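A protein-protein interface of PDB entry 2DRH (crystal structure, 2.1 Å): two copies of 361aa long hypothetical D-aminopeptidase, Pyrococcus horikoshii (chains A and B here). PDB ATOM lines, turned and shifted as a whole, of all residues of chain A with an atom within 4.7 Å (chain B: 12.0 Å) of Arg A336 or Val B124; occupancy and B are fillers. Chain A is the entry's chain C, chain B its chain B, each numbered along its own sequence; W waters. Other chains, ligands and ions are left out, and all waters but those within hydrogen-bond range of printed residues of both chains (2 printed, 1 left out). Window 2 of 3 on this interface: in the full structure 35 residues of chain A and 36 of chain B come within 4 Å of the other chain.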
ATOM      1  N   GLY A  39       0.942  -5.566  24.313  1.00  0.00           N
ATOM      2  CA  GLY A  39       1.245  -6.452  23.208  1.00  0.00           C
ATOM      3  C   GLY A  39       0.538  -6.097  21.919  1.00  0.00           C
ATOM      4  O   GLY A  39       0.112  -4.955  21.719  1.00  0.00           O
ATOM      5  N   LEU A  41      -2.140  -5.669  18.912  1.00  0.00           N
ATOM      6  CA  LEU A  41      -3.479  -5.094  18.962  1.00  0.00           C
ATOM      7  C   LEU A  41      -4.581  -6.125  18.750  1.00  0.00           C
ATOM      8  O   LEU A  41      -4.484  -6.989  17.879  1.00  0.00           O
ATOM      9  CB  LEU A  41      -3.618  -3.991  17.909  1.00  0.00           C
ATOM     10  CG  LEU A  41      -5.010  -3.369  17.757  1.00  0.00           C
ATOM     11  CD1 LEU A  41      -5.430  -2.713  19.070  1.00  0.00           C
ATOM     12  CD2 LEU A  41      -4.996  -2.350  16.624  1.00  0.00           C
ATOM     13  N   PRO A  47      -4.704  -3.535  23.350  1.00  0.00           N
ATOM     14  CA  PRO A  47      -4.546  -2.813  24.622  1.00  0.00           C
ATOM     15  C   PRO A  47      -5.361  -1.522  24.669  1.00  0.00           C
ATOM     16  O   PRO A  47      -5.606  -0.901  23.639  1.00  0.00           O
ATOM     17  CB  PRO A  47      -3.043  -2.541  24.684  1.00  0.00           C
ATOM     18  CG  PRO A  47      -2.454  -3.677  23.886  1.00  0.00           C
ATOM     19  CD  PRO A  47      -3.394  -3.752  22.710  1.00  0.00           C
ATOM     20  N   SER A 139      -5.216   6.446  18.252  1.00  0.00           N
ATOM     21  CA  SER A 139      -4.990   5.148  17.609  1.00  0.00           C
ATOM     22  C   SER A 139      -3.575   4.567  17.701  1.00  0.00           C
ATOM     23  O   SER A 139      -3.410   3.346  17.734  1.00  0.00           O
ATOM     24  CB  SER A 139      -5.389   5.223  16.134  1.00  0.00           C
ATOM     25  OG  SER A 139      -4.562   6.137  15.439  1.00  0.00           O
ATOM     26  N   TYR A 140      -2.559   5.423  17.750  1.00  0.00           N
ATOM     27  CA  TYR A 140      -1.183   4.934  17.796  1.00  0.00           C
ATOM     28  C   TYR A 140      -0.896   4.057  19.012  1.00  0.00           C
ATOM     29  O   TYR A 140      -0.138   3.083  18.922  1.00  0.00           O
ATOM     30  CB  TYR A 140      -0.186   6.099  17.764  1.00  0.00           C
ATOM     31  CG  TYR A 140       1.234   5.644  17.476  1.00  0.00           C
ATOM     32  CD1 TYR A 140       1.620   5.275  16.182  1.00  0.00           C
ATOM     33  CD2 TYR A 140       2.178   5.541  18.498  1.00  0.00           C
ATOM     34  CE1 TYR A 140       2.911   4.814  15.916  1.00  0.00           C
ATOM     35  CE2 TYR A 140       3.474   5.081  18.243  1.00  0.00           C
ATOM     36  CZ  TYR A 140       3.831   4.720  16.949  1.00  0.00           C
ATOM     37  OH  TYR A 140       5.109   4.280  16.690  1.00  0.00           O
ATOM     38  N   LEU A 141      -1.502   4.402  20.145  1.00  0.00           N
ATOM     39  CA  LEU A 141      -1.302   3.647  21.372  1.00  0.00           C
ATOM     40  C   LEU A 141      -2.560   2.931  21.843  1.00  0.00           C
ATOM     41  O   LEU A 141      -2.480   1.906  22.524  1.00  0.00           O
ATOM     42  CB  LEU A 141      -0.820   4.578  22.489  1.00  0.00           C
ATOM     43  CG  LEU A 141       0.539   5.246  22.303  1.00  0.00           C
ATOM     44  CD1 LEU A 141       0.797   6.174  23.478  1.00  0.00           C
ATOM     45  CD2 LEU A 141       1.632   4.183  22.197  1.00  0.00           C
ATOM     46  N   ASN A 142      -3.719   3.467  21.470  1.00  0.00           N
ATOM     47  CA  ASN A 142      -4.993   2.900  21.891  1.00  0.00           C
ATOM     48  C   ASN A 142      -5.792   2.158  20.832  1.00  0.00           C
ATOM     49  O   ASN A 142      -5.705   2.449  19.638  1.00  0.00           O
ATOM     50  CB  ASN A 142      -5.878   4.002  22.481  1.00  0.00           C
ATOM     51  CG  ASN A 142      -7.248   3.492  22.895  1.00  0.00           C
ATOM     52  OD1 ASN A 142      -7.360   2.520  23.638  1.00  0.00           O
ATOM     53  ND2 ASN A 142      -8.294   4.147  22.418  1.00  0.00           N
ATOM     54  N   ARG A 145     -10.741   1.495  17.821  1.00  0.00           N
ATOM     55  CA  ARG A 145     -11.836   0.759  17.213  1.00  0.00           C
ATOM     56  C   ARG A 145     -12.675   0.060  18.288  1.00  0.00           C
ATOM     57  O   ARG A 145     -13.840  -0.274  18.055  1.00  0.00           O
ATOM     58  CB  ARG A 145     -11.300  -0.298  16.249  1.00  0.00           C
ATOM     59  CG  ARG A 145     -10.661   0.239  14.978  1.00  0.00           C
ATOM     60  CD  ARG A 145     -10.198  -0.907  14.091  1.00  0.00           C
ATOM     61  NE  ARG A 145     -11.306  -1.738  13.621  1.00  0.00           N
ATOM     62  CZ  ARG A 145     -12.080  -1.453  12.578  1.00  0.00           C
ATOM     63  NH1 ARG A 145     -11.881  -0.348  11.867  1.00  0.00           N
ATOM     64  NH2 ARG A 145     -13.060  -2.280  12.235  1.00  0.00           N
ATOM     65  N   GLY A 335       1.942   0.778  24.073  1.00  0.00           N
ATOM     66  CA  GLY A 335       0.549   0.499  23.764  1.00  0.00           C
ATOM     67  C   GLY A 335       0.350  -0.552  22.686  1.00  0.00           C
ATOM     68  O   GLY A 335       1.202  -1.414  22.496  1.00  0.00           O
ATOM     69  N   ARG A 336      -0.770  -0.467  21.970  1.00  0.00           N
ATOM     70  CA  ARG A 336      -1.101  -1.432  20.922  1.00  0.00           C
ATOM     71  C   ARG A 336       0.024  -1.708  19.932  1.00  0.00           C
ATOM     72  O   ARG A 336       0.685  -0.790  19.452  1.00  0.00           O
ATOM     73  CB  ARG A 336      -2.364  -0.988  20.174  1.00  0.00           C
ATOM     74  CG  ARG A 336      -2.223   0.258  19.310  1.00  0.00           C
ATOM     75  CD  ARG A 336      -1.883  -0.095  17.867  1.00  0.00           C
ATOM     76  NE  ARG A 336      -2.163   1.018  16.966  1.00  0.00           N
ATOM     77  CZ  ARG A 336      -2.053   0.962  15.644  1.00  0.00           C
ATOM     78  NH1 ARG A 336      -1.666  -0.163  15.045  1.00  0.00           N
ATOM     79  NH2 ARG A 336      -2.339   2.035  14.919  1.00  0.00           N
ATOM     80  N   ASP A 337       0.227  -2.991  19.638  1.00  0.00           N
ATOM     81  CA  ASP A 337       1.271  -3.444  18.723  1.00  0.00           C
ATOM     82  C   ASP A 337       2.657  -3.111  19.252  1.00  0.00           C
ATOM     83  O   ASP A 337       3.627  -3.025  18.494  1.00  0.00           O
ATOM     84  CB  ASP A 337       1.082  -2.834  17.334  1.00  0.00           C
ATOM     85  CG  ASP A 337      -0.124  -3.400  16.622  1.00  0.00           C
ATOM     86  OD1 ASP A 337      -0.356  -4.622  16.739  1.00  0.00           O
ATOM     87  OD2 ASP A 337      -0.836  -2.634  15.945  1.00  0.00           O
ATOM     88  N   ASN A 338       2.735  -2.930  20.566  1.00  0.00           N
ATOM     89  CA  ASN A 338       3.990  -2.614  21.227  1.00  0.00           C
ATOM     90  C   ASN A 338       4.524  -1.236  20.856  1.00  0.00           C
ATOM     91  O   ASN A 338       5.713  -0.968  20.985  1.00  0.00           O
ATOM     92  CB  ASN A 338       5.035  -3.687  20.914  1.00  0.00           C
ATOM     93  CG  ASN A 338       4.686  -5.026  21.523  1.00  0.00           C
ATOM     94  OD1 ASN A 338       4.519  -5.139  22.737  1.00  0.00           O
ATOM     95  ND2 ASN A 338       4.568  -6.050  20.683  1.00  0.00           N
ATOM     96  N   HIS A 339       3.643  -0.364  20.387  1.00  0.00           N
ATOM     97  CA  HIS A 339       4.067   0.984  20.052  1.00  0.00           C
ATOM     98  C   HIS A 339       4.456   1.645  21.364  1.00  0.00           C
ATOM     99  O   HIS A 339       3.970   1.257  22.428  1.00  0.00           O
ATOM    100  CB  HIS A 339       2.926   1.757  19.387  1.00  0.00           C
ATOM    101  CG  HIS A 339       2.694   1.374  17.962  1.00  0.00           C
ATOM    102  ND1 HIS A 339       1.597   1.801  17.245  1.00  0.00           N
ATOM    103  CD2 HIS A 339       3.427   0.617  17.112  1.00  0.00           C
ATOM    104  CE1 HIS A 339       1.665   1.323  16.016  1.00  0.00           C
ATOM    105  NE2 HIS A 339       2.766   0.601  15.909  1.00  0.00           N
ATOM    106  N   TYR B  63     -17.070   5.909   2.566  1.00  0.00           N
ATOM    107  CA  TYR B  63     -15.827   6.309   3.209  1.00  0.00           C
ATOM    108  C   TYR B  63     -14.642   6.186   2.250  1.00  0.00           C
ATOM    109  O   TYR B  63     -13.826   7.101   2.131  1.00  0.00           O
ATOM    110  CB  TYR B  63     -15.584   5.446   4.449  1.00  0.00           C
ATOM    111  CG  TYR B  63     -14.313   5.788   5.192  1.00  0.00           C
ATOM    112  CD1 TYR B  63     -14.194   6.977   5.916  1.00  0.00           C
ATOM    113  CD2 TYR B  63     -13.211   4.937   5.143  1.00  0.00           C
ATOM    114  CE1 TYR B  63     -13.000   7.306   6.571  1.00  0.00           C
ATOM    115  CE2 TYR B  63     -12.025   5.255   5.787  1.00  0.00           C
ATOM    116  CZ  TYR B  63     -11.921   6.436   6.496  1.00  0.00           C
ATOM    117  OH  TYR B  63     -10.728   6.732   7.121  1.00  0.00           O
ATOM    118  N   LYS B  64     -14.552   5.052   1.561  1.00  0.00           N
ATOM    119  CA  LYS B  64     -13.463   4.828   0.615  1.00  0.00           C
ATOM    120  C   LYS B  64     -13.693   5.659  -0.634  1.00  0.00           C
ATOM    121  O   LYS B  64     -12.742   6.089  -1.287  1.00  0.00           O
ATOM    122  CB  LYS B  64     -13.370   3.340   0.262  1.00  0.00           C
ATOM    123  CG  LYS B  64     -12.920   2.486   1.436  1.00  0.00           C
ATOM    124  CD  LYS B  64     -11.487   2.820   1.824  1.00  0.00           C
ATOM    125  CE  LYS B  64     -11.157   2.284   3.202  1.00  0.00           C
ATOM    126  NZ  LYS B  64     -11.466   0.839   3.307  1.00  0.00           N
ATOM    127  N   ILE B 115     -19.944   1.625   9.851  1.00  0.00           N
ATOM    128  CA  ILE B 115     -18.710   2.060   9.204  1.00  0.00           C
ATOM    129  C   ILE B 115     -17.522   1.150   9.476  1.00  0.00           C
ATOM    130  O   ILE B 115     -16.835   0.713   8.547  1.00  0.00           O
ATOM    131  CB  ILE B 115     -18.332   3.487   9.642  1.00  0.00           C
ATOM    132  CG1 ILE B 115     -19.414   4.468   9.186  1.00  0.00           C
ATOM    133  CG2 ILE B 115     -16.978   3.870   9.056  1.00  0.00           C
ATOM    134  CD1 ILE B 115     -19.297   5.850   9.803  1.00  0.00           C
ATOM    135  N   LEU B 116     -17.287   0.871  10.753  1.00  0.00           N
ATOM    136  CA  LEU B 116     -16.173   0.030  11.169  1.00  0.00           C
ATOM    137  C   LEU B 116     -16.243  -1.370  10.578  1.00  0.00           C
ATOM    138  O   LEU B 116     -15.212  -1.968  10.275  1.00  0.00           O
ATOM    139  CB  LEU B 116     -16.128  -0.047  12.698  1.00  0.00           C
ATOM    140  CG  LEU B 116     -16.009   1.327  13.364  1.00  0.00           C
ATOM    141  CD1 LEU B 116     -16.129   1.198  14.874  1.00  0.00           C
ATOM    142  CD2 LEU B 116     -14.678   1.955  12.982  1.00  0.00           C
ATOM    143  N   GLU B 117     -17.455  -1.892  10.415  1.00  0.00           N
ATOM    144  CA  GLU B 117     -17.636  -3.224   9.857  1.00  0.00           C
ATOM    145  C   GLU B 117     -17.266  -3.265   8.386  1.00  0.00           C
ATOM    146  O   GLU B 117     -16.780  -4.280   7.886  1.00  0.00           O
ATOM    147  CB  GLU B 117     -19.082  -3.689  10.026  1.00  0.00           C
ATOM    148  CG  GLU B 117     -19.425  -4.059  11.445  1.00  0.00           C
ATOM    149  CD  GLU B 117     -18.495  -5.116  12.001  1.00  0.00           C
ATOM    150  OE1 GLU B 117     -18.500  -6.250  11.474  1.00  0.00           O
ATOM    151  OE2 GLU B 117     -17.756  -4.810  12.962  1.00  0.00           O
ATOM    152  N   GLU B 118     -17.502  -2.153   7.703  1.00  0.00           N
ATOM    153  CA  GLU B 118     -17.212  -2.043   6.284  1.00  0.00           C
ATOM    154  C   GLU B 118     -15.757  -1.642   6.049  1.00  0.00           C
ATOM    155  O   GLU B 118     -15.227  -1.807   4.950  1.00  0.00           O
ATOM    156  CB  GLU B 118     -18.136  -1.004   5.648  1.00  0.00           C
ATOM    157  CG  GLU B 118     -19.617  -1.202   5.951  1.00  0.00           C
ATOM    158  CD  GLU B 118     -20.148  -2.545   5.475  1.00  0.00           C
ATOM    159  OE1 GLU B 118     -19.926  -2.893   4.293  1.00  0.00           O
ATOM    160  OE2 GLU B 118     -20.799  -3.246   6.284  1.00  0.00           O
ATOM    161  N   ASN B 119     -15.106  -1.132   7.089  1.00  0.00           N
ATOM    162  CA  ASN B 119     -13.719  -0.699   6.969  1.00  0.00           C
ATOM    163  C   ASN B 119     -12.918  -1.042   8.222  1.00  0.00           C
ATOM    164  O   ASN B 119     -12.894  -0.270   9.181  1.00  0.00           O
ATOM    165  CB  ASN B 119     -13.673   0.814   6.730  1.00  0.00           C
ATOM    166  CG  ASN B 119     -14.489   1.240   5.521  1.00  0.00           C
ATOM    167  OD1 ASN B 119     -14.083   1.033   4.376  1.00  0.00           O
ATOM    168  ND2 ASN B 119     -15.654   1.830   5.772  1.00  0.00           N
ATOM    169  N   GLU B 120     -12.250  -2.192   8.211  1.00  0.00           N
ATOM    170  CA  GLU B 120     -11.464  -2.613   9.367  1.00  0.00           C
ATOM    171  C   GLU B 120     -10.094  -1.930   9.413  1.00  0.00           C
ATOM    172  O   GLU B 120      -9.333  -2.118  10.358  1.00  0.00           O
ATOM    173  CB  GLU B 120     -11.303  -4.140   9.364  1.00  0.00           C
ATOM    174  CG  GLU B 120     -10.454  -4.685   8.226  1.00  0.00           C
ATOM    175  CD  GLU B 120     -10.578  -6.193   8.072  1.00  0.00           C
ATOM    176  OE1 GLU B 120     -10.702  -6.894   9.101  1.00  0.00           O
ATOM    177  OE2 GLU B 120     -10.540  -6.678   6.920  1.00  0.00           O
ATOM    178  N   ASP B 121      -9.792  -1.126   8.398  1.00  0.00           N
ATOM    179  CA  ASP B 121      -8.516  -0.414   8.342  1.00  0.00           C
ATOM    180  C   ASP B 121      -8.553   0.907   9.115  1.00  0.00           C
ATOM    181  O   ASP B 121      -7.510   1.472   9.445  1.00  0.00           O
ATOM    182  CB  ASP B 121      -8.101  -0.177   6.879  1.00  0.00           C
ATOM    183  CG  ASP B 121      -9.172   0.534   6.061  1.00  0.00           C
ATOM    184  OD1 ASP B 121     -10.374   0.374   6.365  1.00  0.00           O
ATOM    185  OD2 ASP B 121      -8.807   1.242   5.093  1.00  0.00           O
ATOM    186  N   ILE B 122      -9.758   1.382   9.415  1.00  0.00           N
ATOM    187  CA  ILE B 122      -9.944   2.627  10.166  1.00  0.00           C
ATOM    188  C   ILE B 122      -9.447   2.483  11.605  1.00  0.00           C
ATOM    189  O   ILE B 122      -9.836   1.556  12.307  1.00  0.00           O
ATOM    190  CB  ILE B 122     -11.441   3.036  10.194  1.00  0.00           C
ATOM    191  CG1 ILE B 122     -11.863   3.545   8.818  1.00  0.00           C
ATOM    192  CG2 ILE B 122     -11.687   4.082  11.272  1.00  0.00           C
ATOM    193  CD1 ILE B 122     -13.322   3.954   8.728  1.00  0.00           C
ATOM    194  N   GLY B 123      -8.584   3.405  12.033  1.00  0.00           N
ATOM    195  CA  GLY B 123      -8.058   3.377  13.390  1.00  0.00           C
ATOM    196  C   GLY B 123      -6.864   2.463  13.613  1.00  0.00           C
ATOM    197  O   GLY B 123      -6.392   2.302  14.743  1.00  0.00           O
ATOM    198  N   VAL B 124      -6.365   1.873  12.531  1.00  0.00           N
ATOM    199  CA  VAL B 124      -5.233   0.960  12.605  1.00  0.00           C
ATOM    200  C   VAL B 124      -4.197   1.309  11.544  1.00  0.00           C
ATOM    201  O   VAL B 124      -3.072   1.689  11.868  1.00  0.00           O
ATOM    202  CB  VAL B 124      -5.700  -0.500  12.405  1.00  0.00           C
ATOM    203  CG1 VAL B 124      -4.519  -1.452  12.477  1.00  0.00           C
ATOM    204  CG2 VAL B 124      -6.725  -0.854  13.461  1.00  0.00           C
ATOM    205  N   THR B 125      -4.576   1.185  10.278  1.00  0.00           N
ATOM    206  CA  THR B 125      -3.660   1.494   9.188  1.00  0.00           C
ATOM    207  C   THR B 125      -4.027   2.784   8.455  1.00  0.00           C
ATOM    208  O   THR B 125      -3.295   3.235   7.572  1.00  0.00           O
ATOM    209  CB  THR B 125      -3.591   0.336   8.178  1.00  0.00           C
ATOM    210  OG1 THR B 125      -4.903   0.045   7.689  1.00  0.00           O
ATOM    211  CG2 THR B 125      -3.025  -0.896   8.841  1.00  0.00           C
ATOM    212  N   THR B 126      -5.166   3.369   8.810  1.00  0.00           N
ATOM    213  CA  THR B 126      -5.577   4.627   8.200  1.00  0.00           C
ATOM    214  C   THR B 126      -6.150   5.555   9.269  1.00  0.00           C
ATOM    215  O   THR B 126      -6.058   5.275  10.468  1.00  0.00           O
ATOM    216  CB  THR B 126      -6.621   4.422   7.079  1.00  0.00           C
ATOM    217  OG1 THR B 126      -6.667   5.599   6.265  1.00  0.00           O
ATOM    218  CG2 THR B 126      -8.002   4.180   7.659  1.00  0.00           C
ATOM    219  N   GLY B 127      -6.747   6.657   8.831  1.00  0.00           N
ATOM    220  CA  GLY B 127      -7.289   7.618   9.769  1.00  0.00           C
ATOM    221  C   GLY B 127      -8.637   7.286  10.370  1.00  0.00           C
ATOM    222  O   GLY B 127      -9.138   6.170  10.260  1.00  0.00           O
ATOM    223  N   SER B 128      -9.216   8.301  11.001  1.00  0.00           N
ATOM    224  CA  SER B 128     -10.503   8.239  11.673  1.00  0.00           C
ATOM    225  C   SER B 128     -11.632   8.343  10.651  1.00  0.00           C
ATOM    226  O   SER B 128     -11.411   8.156   9.450  1.00  0.00           O
ATOM    227  CB  SER B 128     -10.577   9.407  12.667  1.00  0.00           C
ATOM    228  OG  SER B 128     -11.824   9.467  13.326  1.00  0.00           O
ATOM    229  N   VAL B 129     -12.840   8.640  11.124  1.00  0.00           N
ATOM    230  CA  VAL B 129     -13.991   8.793  10.237  1.00  0.00           C
ATOM    231  C   VAL B 129     -14.925   9.887  10.750  1.00  0.00           C
ATOM    232  O   VAL B 129     -15.074  10.076  11.965  1.00  0.00           O
ATOM    233  CB  VAL B 129     -14.772   7.465  10.072  1.00  0.00           C
ATOM    234  CG1 VAL B 129     -15.176   6.906  11.426  1.00  0.00           C
ATOM    235  CG2 VAL B 129     -15.985   7.694   9.195  1.00  0.00           C
ATOM    236  N   HIS B 292     -10.343   7.757  -1.027  1.00  0.00           N
ATOM    237  CA  HIS B 292      -9.682   7.969   0.262  1.00  0.00           C
ATOM    238  C   HIS B 292      -8.160   7.903   0.166  1.00  0.00           C
ATOM    239  O   HIS B 292      -7.460   8.745   0.727  1.00  0.00           O
ATOM    240  CB  HIS B 292     -10.173   6.922   1.272  1.00  0.00           C
ATOM    241  CG  HIS B 292      -9.628   7.097   2.658  1.00  0.00           C
ATOM    242  ND1 HIS B 292     -10.048   8.103   3.503  1.00  0.00           N
ATOM    243  CD2 HIS B 292      -8.706   6.387   3.349  1.00  0.00           C
ATOM    244  CE1 HIS B 292      -9.410   8.002   4.657  1.00  0.00           C
ATOM    245  NE2 HIS B 292      -8.589   6.969   4.589  1.00  0.00           N
ATOM    246  N   TYR B 293      -7.652   6.907  -0.555  1.00  0.00           N
ATOM    247  CA  TYR B 293      -6.212   6.713  -0.691  1.00  0.00           C
ATOM    248  C   TYR B 293      -5.519   7.398  -1.874  1.00  0.00           C
ATOM    249  O   TYR B 293      -4.302   7.274  -2.027  1.00  0.00           O
ATOM    250  CB  TYR B 293      -5.902   5.211  -0.718  1.00  0.00           C
ATOM    251  CG  TYR B 293      -6.065   4.534   0.626  1.00  0.00           C
ATOM    252  CD1 TYR B 293      -5.199   4.819   1.680  1.00  0.00           C
ATOM    253  CD2 TYR B 293      -7.084   3.612   0.842  1.00  0.00           C
ATOM    254  CE1 TYR B 293      -5.345   4.203   2.919  1.00  0.00           C
ATOM    255  CE2 TYR B 293      -7.238   2.986   2.080  1.00  0.00           C
ATOM    256  CZ  TYR B 293      -6.364   3.286   3.111  1.00  0.00           C
ATOM    257  OH  TYR B 293      -6.504   2.668   4.332  1.00  0.00           O
HETATM  258  O   HOH W   1      -6.590   6.343  13.133  1.00  0.00           O
HETATM  259  O   HOH W   2      -0.839  -0.595  12.469  1.00  0.00           O
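The guanidinium group (NH1) of Arg A145 is in hydrogen-bond range of the backbone carbonyl oxygen (O) of Ile B122.
The guanidinium group (NH2) of Arg A145 sits at hydrogen-bond distance from the backbone carbonyl oxygen (O) of Leu B116, 2.9 Å away.
The backbone carbonyl oxygen of Asn B119 sits at hydrogen-bond distance from the guanidinium group of Arg A145 (2.9 Å).
The guanidinium group of Arg A145 sits close to the backbone carbonyl oxygen of Glu B120 (3.4 Å).
NH2 of Arg A336 lies within hydrogen-bond range of O of Val B124, 3.2 Å away.
NZ of Lys B64 is in hydrogen-bond range of OD1 of Asn B119 (2.8 Å).
The side-chain carboxylate (OD2) of Asp A337 lies within salt-bridge range of the guanidinium group (NH1) of Arg A336 (2.8 Å).
The side-chain amide nitrogen of Asn B119 sits at hydrogen-bond distance from the backbone carbonyl oxygen of Ile B115, 3.2 Å away.
The backbone NH (N) of Leu A41 sits at hydrogen-bond distance from the side-chain carboxylate (OD1) of Asp A337, at 3.0 Å.
The backbone NH of Arg A336 sits at hydrogen-bond distance from the backbone carbonyl oxygen of Leu A141 (3.0 Å).
O of Tyr A140 is in hydrogen-bond range of NE of Arg A336.
Among the printed residues, merely in contact across the chains: Ser A139 with Gly B123 (3.4 Å), Arg A145 with Val B124 (3.5 Å) and Leu A41 with Val B124 (3.9 Å).
No residue of chain B comes within 4 Å of Gly A39.
Leu A41 touches just one residue of chain B: Val B124.
No residue of chain B comes within 4 Å of Leu A141.
Asn A142 touches none of the printed residues of chain B.
Of the printed residues of chain B, Arg A145 touches Leu B116, Asn B119, Glu B120, Ile B122 and Val B124.
No residue of chain B comes within 4 Å of Asp A337.
No residue of chain B comes within 4 Å of Asn A338.
No residue of chain B comes within 4 Å of His A339.
Of the printed residues of chain A, Asn B119 touches Arg A145.
Of the printed residues of chain A, Glu B120 touches Arg A145 (3.3 Å).
Of the printed residues of chain A, Ile B122 touches Arg A145 (2.8 Å).
Printed residues of chain A within 4 Å of Val B124: Leu A41, Arg A145 and Arg A336.
Ser B128 touches none of the printed residues of chain A.
Hydrophobic or aromatic side chains of chain A within 4 Å of the printed part of chain B: Leu A41.
Of the 19 printed residues of chain B, 6 touch a printed residue of chain A.
No position is printed for both chains.
Water W2 bridges the guanidinium group (NH1) of Arg A336 (2.7 Å) and the backbone carbonyl oxygen (O) of Val B124 (3.3 Å).
Water W1 bridges the backbone carbonyl oxygen (O) of Thr B126 and the side-chain hydroxyl (OG) of Ser A139.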
